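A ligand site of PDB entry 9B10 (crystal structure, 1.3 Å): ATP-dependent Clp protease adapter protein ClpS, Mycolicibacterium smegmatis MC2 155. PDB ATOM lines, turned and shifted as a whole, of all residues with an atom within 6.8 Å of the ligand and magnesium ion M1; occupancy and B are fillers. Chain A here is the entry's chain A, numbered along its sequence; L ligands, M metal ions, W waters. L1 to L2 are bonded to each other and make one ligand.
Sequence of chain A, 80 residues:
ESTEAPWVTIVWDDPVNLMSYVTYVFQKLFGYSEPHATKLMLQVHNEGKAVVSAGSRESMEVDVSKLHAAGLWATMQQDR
Water W2 binds magnesium ion M1, at 2.0 Å. Magnesium ion M1 is bound by water W4 (2.1 Å). Magnesium ion M1 is bound by water W1, 2.1 Å away. Magnesium ion M1 is bound by a ring nitrogen (NE2) of His 45 (2.2 Å). Magnesium ion M1 is bound by N1 of LIG L1. Magnesium ion M1 is bound by an oxygen (O1) of LIG L1, 2.3 Å away.
O of Val 16 sits at hydrogen-bond distance from N2 of LG2 L2 (2.7 Å). A nitrogen (N1) of LIG L1 lies close to the backbone carbonyl oxygen of Asp 14. The side-chain carboxylate (OD1) of Asp 13 sits close to a nitrogen (N1) of LIG L1, 3.1 Å away. The backbone NH of Met 19 is in hydrogen-bond range of an oxygen (O1) of LG2 L2. N1 of LG2 L2 is in hydrogen-bond range of O of Asn 17 (2.8 Å).
The side-chain carboxylate (OD1) of Asp 14 is in hydrogen-bond range of the backbone NH (N) of Val 16, 2.9 Å away. The backbone NH (N) of Trp 12 sits at hydrogen-bond distance from the backbone carbonyl oxygen (O) of Trp 73. OD2 of Asp 14 sits close to OD1 of Asn 17, at 2.8 Å. ND1 of His 45 is in hydrogen-bond range of SD of Met 19 (3.7 Å).
Residues that only touch the ligand: Val 11 (3.3 Å), Pro 15 (3.3 Å), Val 44 (3.4 Å), Leu 18 (3.4 Å), Val 22 (3.5 Å) and Trp 12 (3.6 Å). Hydrophobic or aromatic side chains that line the ligand: Val 11, Leu 18, Met 19, Val 22, Val 44 and His 45. Within 4 Å of the ligand: Val 11, Trp 12, Asp 13, Asp 14, Pro 15, Val 16, Asn 17, Leu 18, Met 19, Val 22, Val 44 and His 45. Along chain A the residues within 4 Å of the ligand span positions 11 to 45.
One residue has an atom within 4 Å of magnesium ion M1: His 45.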
ATOM      1  N   VAL A  11      -2.541   2.312   9.166  1.00  0.00           N
ATOM      2  CA  VAL A  11      -2.826   3.002   7.917  1.00  0.00           C
ATOM      3  C   VAL A  11      -1.710   4.002   7.670  1.00  0.00           C
ATOM      4  O   VAL A  11      -1.273   4.710   8.578  1.00  0.00           O
ATOM      5  CB  VAL A  11      -4.215   3.658   7.931  1.00  0.00           C
ATOM      6  CG1 VAL A  11      -4.409   4.553   6.710  1.00  0.00           C
ATOM      7  CG2 VAL A  11      -5.261   2.573   7.953  1.00  0.00           C
ATOM      8  N   TRP A  12      -1.245   4.040   6.417  1.00  0.00           N
ATOM      9  CA  TRP A  12      -0.112   4.847   5.992  1.00  0.00           C
ATOM     10  C   TRP A  12      -0.593   5.979   5.107  1.00  0.00           C
ATOM     11  O   TRP A  12      -1.463   5.790   4.256  1.00  0.00           O
ATOM     12  CB  TRP A  12       0.863   3.989   5.187  1.00  0.00           C
ATOM     13  CG  TRP A  12       1.418   2.857   5.964  1.00  0.00           C
ATOM     14  CD1 TRP A  12       0.846   1.635   6.162  1.00  0.00           C
ATOM     15  CD2 TRP A  12       2.661   2.835   6.668  1.00  0.00           C
ATOM     16  NE1 TRP A  12       1.657   0.856   6.940  1.00  0.00           N
ATOM     17  CE2 TRP A  12       2.785   1.573   7.267  1.00  0.00           C
ATOM     18  CE3 TRP A  12       3.690   3.759   6.837  1.00  0.00           C
ATOM     19  CZ2 TRP A  12       3.895   1.204   8.023  1.00  0.00           C
ATOM     20  CZ3 TRP A  12       4.790   3.401   7.584  1.00  0.00           C
ATOM     21  CH2 TRP A  12       4.882   2.135   8.179  1.00  0.00           C
ATOM     22  N   ASP A  13      -0.023   7.168   5.299  1.00  0.00           N
ATOM     23  CA  ASP A  13      -0.422   8.331   4.504  1.00  0.00           C
ATOM     24  C   ASP A  13      -0.147   8.072   3.027  1.00  0.00           C
ATOM     25  O   ASP A  13       0.865   7.467   2.671  1.00  0.00           O
ATOM     26  CB  ASP A  13       0.368   9.554   4.979  1.00  0.00           C
ATOM     27  CG  ASP A  13      -0.110  10.832   4.325  1.00  0.00           C
ATOM     28  OD1 ASP A  13      -1.337  11.006   4.198  1.00  0.00           O
ATOM     29  OD2 ASP A  13       0.742  11.651   3.946  1.00  0.00           O
ATOM     30  N   ASP A  14      -1.036   8.540   2.171  1.00  0.00           N
ATOM     31  CA  ASP A  14      -0.849   8.409   0.740  1.00  0.00           C
ATOM     32  C   ASP A  14      -1.243   9.713   0.073  1.00  0.00           C
ATOM     33  O   ASP A  14      -2.014  10.502   0.640  1.00  0.00           O
ATOM     34  CB  ASP A  14      -1.610   7.207   0.164  1.00  0.00           C
ATOM     35  CG  ASP A  14      -3.093   7.454  -0.031  1.00  0.00           C
ATOM     36  OD1 ASP A  14      -3.426   8.191  -0.995  1.00  0.00           O
ATOM     37  OD2 ASP A  14      -3.903   6.905   0.736  1.00  0.00           O
ATOM     38  N   PRO A  15      -0.701  10.005  -1.112  1.00  0.00           N
ATOM     39  CA  PRO A  15      -0.899  11.332  -1.699  1.00  0.00           C
ATOM     40  C   PRO A  15      -2.179  11.506  -2.496  1.00  0.00           C
ATOM     41  O   PRO A  15      -2.437  12.623  -2.977  1.00  0.00           O
ATOM     42  CB  PRO A  15       0.321  11.457  -2.634  1.00  0.00           C
ATOM     43  CG  PRO A  15       0.624  10.059  -3.036  1.00  0.00           C
ATOM     44  CD  PRO A  15       0.296   9.212  -1.843  1.00  0.00           C
ATOM     45  N   VAL A  16      -2.987  10.469  -2.662  1.00  0.00           N
ATOM     46  CA  VAL A  16      -4.156  10.512  -3.523  1.00  0.00           C
ATOM     47  C   VAL A  16      -5.447  10.676  -2.733  1.00  0.00           C
ATOM     48  O   VAL A  16      -6.274  11.523  -3.062  1.00  0.00           O
ATOM     49  CB  VAL A  16      -4.211   9.255  -4.426  1.00  0.00           C
ATOM     50  CG1 VAL A  16      -5.462   9.272  -5.299  1.00  0.00           C
ATOM     51  CG2 VAL A  16      -2.960   9.174  -5.292  1.00  0.00           C
ATOM     52  N   ASN A  17      -5.637   9.871  -1.695  1.00  0.00           N
ATOM     53  CA  ASN A  17      -6.924   9.865  -1.011  1.00  0.00           C
ATOM     54  C   ASN A  17      -7.204  11.203  -0.351  1.00  0.00           C
ATOM     55  O   ASN A  17      -6.313  11.871   0.163  1.00  0.00           O
ATOM     56  CB  ASN A  17      -6.975   8.750   0.023  1.00  0.00           C
ATOM     57  CG  ASN A  17      -7.246   7.414  -0.593  1.00  0.00           C
ATOM     58  OD1 ASN A  17      -6.438   6.492  -0.481  1.00  0.00           O
ATOM     59  ND2 ASN A  17      -8.392   7.283  -1.242  1.00  0.00           N
ATOM     60  N   LEU A  18      -8.482  11.581  -0.368  1.00  0.00           N
ATOM     61  CA  LEU A  18      -8.925  12.777   0.337  1.00  0.00           C
ATOM     62  C   LEU A  18      -8.972  12.531   1.835  1.00  0.00           C
ATOM     63  O   LEU A  18      -9.418  11.475   2.288  1.00  0.00           O
ATOM     64  CB  LEU A  18     -10.331  13.160  -0.141  1.00  0.00           C
ATOM     65  CG  LEU A  18     -10.446  13.686  -1.563  1.00  0.00           C
ATOM     66  CD1 LEU A  18     -11.899  13.628  -2.027  1.00  0.00           C
ATOM     67  CD2 LEU A  18      -9.932  15.117  -1.640  1.00  0.00           C
ATOM     68  N   MET A  19      -8.549  13.534   2.600  1.00  0.00           N
ATOM     69  CA  MET A  19      -8.744  13.497   4.047  1.00  0.00           C
ATOM     70  C   MET A  19     -10.187  13.175   4.394  1.00  0.00           C
ATOM     71  O   MET A  19     -10.448  12.374   5.306  1.00  0.00           O
ATOM     72  CB  MET A  19      -8.374  14.857   4.642  1.00  0.00           C
ATOM     73  CG  MET A  19      -6.909  15.215   4.526  1.00  0.00           C
ATOM     74  SD  MET A  19      -6.568  16.881   5.104  1.00  0.00           S
ATOM     75  CE  MET A  19      -7.379  17.873   3.850  1.00  0.00           C
ATOM     76  N   SER A  20     -11.140  13.801   3.713  1.00  0.00           N
ATOM     77  CA  SER A  20     -12.545  13.590   4.045  1.00  0.00           C
ATOM     78  C   SER A  20     -12.938  12.143   3.798  1.00  0.00           C
ATOM     79  O   SER A  20     -13.726  11.572   4.559  1.00  0.00           O
ATOM     80  CB  SER A  20     -13.415  14.536   3.225  1.00  0.00           C
ATOM     81  OG  SER A  20     -13.273  14.266   1.838  1.00  0.00           O
ATOM     82  N   TYR A  21     -12.418  11.542   2.726  1.00  0.00           N
ATOM     83  CA  TYR A  21     -12.716  10.155   2.429  1.00  0.00           C
ATOM     84  C   TYR A  21     -12.189   9.239   3.518  1.00  0.00           C
ATOM     85  O   TYR A  21     -12.874   8.304   3.953  1.00  0.00           O
ATOM     86  CB  TYR A  21     -12.099   9.770   1.082  1.00  0.00           C
ATOM     87  CG  TYR A  21     -12.341   8.334   0.714  1.00  0.00           C
ATOM     88  CD1 TYR A  21     -13.623   7.869   0.485  1.00  0.00           C
ATOM     89  CD2 TYR A  21     -11.278   7.447   0.575  1.00  0.00           C
ATOM     90  CE1 TYR A  21     -13.851   6.552   0.136  1.00  0.00           C
ATOM     91  CE2 TYR A  21     -11.503   6.136   0.218  1.00  0.00           C
ATOM     92  CZ  TYR A  21     -12.790   5.698   0.004  1.00  0.00           C
ATOM     93  OH  TYR A  21     -13.018   4.382  -0.345  1.00  0.00           O
ATOM     94  N   VAL A  22     -10.962   9.483   3.972  1.00  0.00           N
ATOM     95  CA  VAL A  22     -10.335   8.631   4.980  1.00  0.00           C
ATOM     96  C   VAL A  22     -11.146   8.667   6.279  1.00  0.00           C
ATOM     97  O   VAL A  22     -11.392   7.624   6.894  1.00  0.00           O
ATOM     98  CB  VAL A  22      -8.867   9.037   5.183  1.00  0.00           C
ATOM     99  CG1 VAL A  22      -8.247   8.273   6.343  1.00  0.00           C
ATOM    100  CG2 VAL A  22      -8.086   8.804   3.910  1.00  0.00           C
ATOM    101  N   PHE A  26     -12.981   5.292   7.983  1.00  0.00           N
ATOM    102  CA  PHE A  26     -12.832   4.795   9.350  1.00  0.00           C
ATOM    103  C   PHE A  26     -14.187   4.661  10.051  1.00  0.00           C
ATOM    104  O   PHE A  26     -14.400   3.707  10.811  1.00  0.00           O
ATOM    105  CB  PHE A  26     -11.893   5.721  10.147  1.00  0.00           C
ATOM    106  CG  PHE A  26     -10.454   5.711   9.663  1.00  0.00           C
ATOM    107  CD1 PHE A  26      -9.942   4.683   8.878  1.00  0.00           C
ATOM    108  CD2 PHE A  26      -9.608   6.740  10.013  1.00  0.00           C
ATOM    109  CE1 PHE A  26      -8.615   4.703   8.469  1.00  0.00           C
ATOM    110  CE2 PHE A  26      -8.289   6.764   9.615  1.00  0.00           C
ATOM    111  CZ  PHE A  26      -7.796   5.744   8.841  1.00  0.00           C
ATOM    112  N   LEU A  40      -7.859   9.964  14.006  1.00  0.00           N
ATOM    113  CA  LEU A  40      -7.003   8.922  13.375  1.00  0.00           C
ATOM    114  C   LEU A  40      -6.545   9.409  11.992  1.00  0.00           C
ATOM    115  O   LEU A  40      -5.386   9.224  11.686  1.00  0.00           O
ATOM    116  CB  LEU A  40      -7.767   7.603  13.273  1.00  0.00           C
ATOM    117  CG  LEU A  40      -7.969   6.836  14.580  1.00  0.00           C
ATOM    118  CD1 LEU A  40      -8.819   5.598  14.320  1.00  0.00           C
ATOM    119  CD2 LEU A  40      -6.653   6.465  15.229  1.00  0.00           C
ATOM    120  N   MET A  41      -7.450   9.977  11.194  1.00  0.00           N
ATOM    121  CA  MET A  41      -7.062  10.463   9.871  1.00  0.00           C
ATOM    122  C   MET A  41      -5.963  11.509   9.982  1.00  0.00           C
ATOM    123  O   MET A  41      -4.985  11.473   9.237  1.00  0.00           O
ATOM    124  CB  MET A  41      -8.296  11.014   9.156  1.00  0.00           C
ATOM    125  CG  MET A  41      -8.006  11.635   7.792  1.00  0.00           C
ATOM    126  SD  MET A  41      -7.364  13.327   7.856  1.00  0.00           S
ATOM    127  CE  MET A  41      -8.846  14.206   8.374  1.00  0.00           C
ATOM    128  N   LEU A  42      -6.113  12.445  10.927  1.00  0.00           N
ATOM    129  CA  LEU A  42      -5.118  13.499  11.090  1.00  0.00           C
ATOM    130  C   LEU A  42      -3.798  12.938  11.620  1.00  0.00           C
ATOM    131  O   LEU A  42      -2.731  13.444  11.253  1.00  0.00           O
ATOM    132  CB  LEU A  42      -5.650  14.597  11.998  1.00  0.00           C
ATOM    133  CG  LEU A  42      -6.794  15.409  11.409  1.00  0.00           C
ATOM    134  CD1 LEU A  42      -7.456  16.278  12.469  1.00  0.00           C
ATOM    135  CD2 LEU A  42      -6.304  16.277  10.255  1.00  0.00           C
ATOM    136  N   VAL A  44      -2.595   9.939  10.850  1.00  0.00           N
ATOM    137  CA  VAL A  44      -1.968   9.433   9.629  1.00  0.00           C
ATOM    138  C   VAL A  44      -1.361  10.594   8.845  1.00  0.00           C
ATOM    139  O   VAL A  44      -0.208  10.530   8.388  1.00  0.00           O
ATOM    140  CB  VAL A  44      -2.982   8.669   8.757  1.00  0.00           C
ATOM    141  CG1 VAL A  44      -2.331   8.248   7.451  1.00  0.00           C
ATOM    142  CG2 VAL A  44      -3.528   7.456   9.482  1.00  0.00           C
ATOM    143  N   HIS A  45      -2.138  11.656   8.672  1.00  0.00           N
ATOM    144  CA  HIS A  45      -1.709  12.729   7.787  1.00  0.00           C
ATOM    145  C   HIS A  45      -0.507  13.471   8.346  1.00  0.00           C
ATOM    146  O   HIS A  45       0.405  13.853   7.588  1.00  0.00           O
ATOM    147  CB  HIS A  45      -2.844  13.702   7.515  1.00  0.00           C
ATOM    148  CG  HIS A  45      -2.708  14.429   6.219  1.00  0.00           C
ATOM    149  ND1 HIS A  45      -3.210  15.690   6.006  1.00  0.00           N
ATOM    150  CD2 HIS A  45      -2.120  14.059   5.058  1.00  0.00           C
ATOM    151  CE1 HIS A  45      -2.928  16.069   4.774  1.00  0.00           C
ATOM    152  NE2 HIS A  45      -2.278  15.095   4.178  1.00  0.00           N
ATOM    153  N   LEU A  72      -7.259   2.372   0.830  1.00  0.00           N
ATOM    154  CA  LEU A  72      -6.281   2.916   1.749  1.00  0.00           C
ATOM    155  C   LEU A  72      -5.092   1.978   1.890  1.00  0.00           C
ATOM    156  O   LEU A  72      -5.180   0.774   1.655  1.00  0.00           O
ATOM    157  CB  LEU A  72      -6.914   3.187   3.118  1.00  0.00           C
ATOM    158  CG  LEU A  72      -8.126   4.112   3.147  1.00  0.00           C
ATOM    159  CD1 LEU A  72      -8.455   4.498   4.571  1.00  0.00           C
ATOM    160  CD2 LEU A  72      -7.908   5.363   2.291  1.00  0.00           C
ATOM    161  N   TRP A  73      -3.955   2.557   2.270  1.00  0.00           N
ATOM    162  CA  TRP A  73      -2.715   1.805   2.437  1.00  0.00           C
ATOM    163  C   TRP A  73      -2.682   1.290   3.871  1.00  0.00           C
ATOM    164  O   TRP A  73      -2.470   2.075   4.801  1.00  0.00           O
ATOM    165  CB  TRP A  73      -1.499   2.679   2.186  1.00  0.00           C
ATOM    166  CG  TRP A  73      -1.334   3.173   0.791  1.00  0.00           C
ATOM    167  CD1 TRP A  73      -2.155   2.940  -0.268  1.00  0.00           C
ATOM    168  CD2 TRP A  73      -0.276   4.008   0.317  1.00  0.00           C
ATOM    169  NE1 TRP A  73      -1.660   3.589  -1.383  1.00  0.00           N
ATOM    170  CE2 TRP A  73      -0.511   4.252  -1.045  1.00  0.00           C
ATOM    171  CE3 TRP A  73       0.837   4.587   0.925  1.00  0.00           C
ATOM    172  CZ2 TRP A  73       0.331   5.040  -1.822  1.00  0.00           C
ATOM    173  CZ3 TRP A  73       1.676   5.369   0.155  1.00  0.00           C
ATOM    174  CH2 TRP A  73       1.422   5.590  -1.204  1.00  0.00           C
HETATM  175  N1  LIG L   1      -2.569  12.700   1.923  1.00  0.00           N
HETATM  176  C1  LIG L   1      -4.024  12.945   1.826  1.00  0.00           C
HETATM  177  C2  LIG L   1      -4.280  14.349   1.240  1.00  0.00           C
HETATM  178  O1  LIG L   1      -3.637  15.337   1.571  1.00  0.00           O
HETATM  179  C3  LIG L   1      -4.756  12.749   3.146  1.00  0.00           C
HETATM  180  C4  LIG L   1      -4.703  11.311   3.668  1.00  0.00           C
HETATM  181  C5  LIG L   1      -4.575  10.225   2.794  1.00  0.00           C
HETATM  182  C6  LIG L   1      -4.787  11.035   5.020  1.00  0.00           C
HETATM  183  C7  LIG L   1      -4.544   8.932   3.262  1.00  0.00           C
HETATM  184  C8  LIG L   1      -4.751   9.740   5.500  1.00  0.00           C
HETATM  185  C9  LIG L   1      -4.626   8.680   4.618  1.00  0.00           C
HETATM  186  O2  LIG L   1      -4.596   7.401   5.080  1.00  0.00           O
HETATM  187  N1  LG2 L   2      -5.275  14.452   0.398  1.00  0.00           N
HETATM  188  C1  LG2 L   2      -5.587  15.731  -0.277  1.00  0.00           C
HETATM  189  C2  LG2 L   2      -6.748  16.460   0.398  1.00  0.00           C
HETATM  190  O1  LG2 L   2      -7.539  15.804   1.042  1.00  0.00           O
HETATM  191  C3  LG2 L   2      -5.992  15.381  -1.707  1.00  0.00           C
HETATM  192  C4  LG2 L   2      -4.824  14.868  -2.542  1.00  0.00           C
HETATM  193  C5  LG2 L   2      -5.175  14.900  -4.009  1.00  0.00           C
HETATM  194  N2  LG2 L   2      -6.230  13.934  -4.339  1.00  0.00           N
HETATM  195  C6  LG2 L   2      -7.494  14.217  -4.600  1.00  0.00           C
HETATM  196  N3  LG2 L   2      -7.880  15.462  -4.801  1.00  0.00           N
HETATM  197  N4  LG2 L   2      -8.380  13.251  -4.688  1.00  0.00           N
HETATM  198  O2  LG2 L   2      -6.844  17.643   0.222  1.00  0.00           O
HETATM  199 MG    MG M   1      -1.463  14.697   2.165  1.00  0.00          MG
HETATM  200 MG    MG M   2      -3.868   5.432   3.013  1.00  0.00          MG
HETATM  201  O   HOH W   1      -0.640  14.428   0.200  1.00  0.00           O
HETATM  202  O   HOH W   2       0.262  14.147   3.039  1.00  0.00           O
HETATM  203  O   HOH W   3      -9.195  18.703  -0.214  1.00  0.00           O
HETATM  204  O   HOH W   4      -0.851  16.698   2.376  1.00  0.00           O
HETATM  205  O   HOH W   5      -5.193  19.001  -1.659  1.00  0.00           O
HETATM  206  O   HOH W   6      -2.453  16.929  -4.353  1.00  0.00           O
HETATM  207  O   HOH W   7     -11.144  13.264  -5.514  1.00  0.00           O
HETATM  208  O   HOH W   8      -1.421  14.825  -2.330  1.00  0.00           O
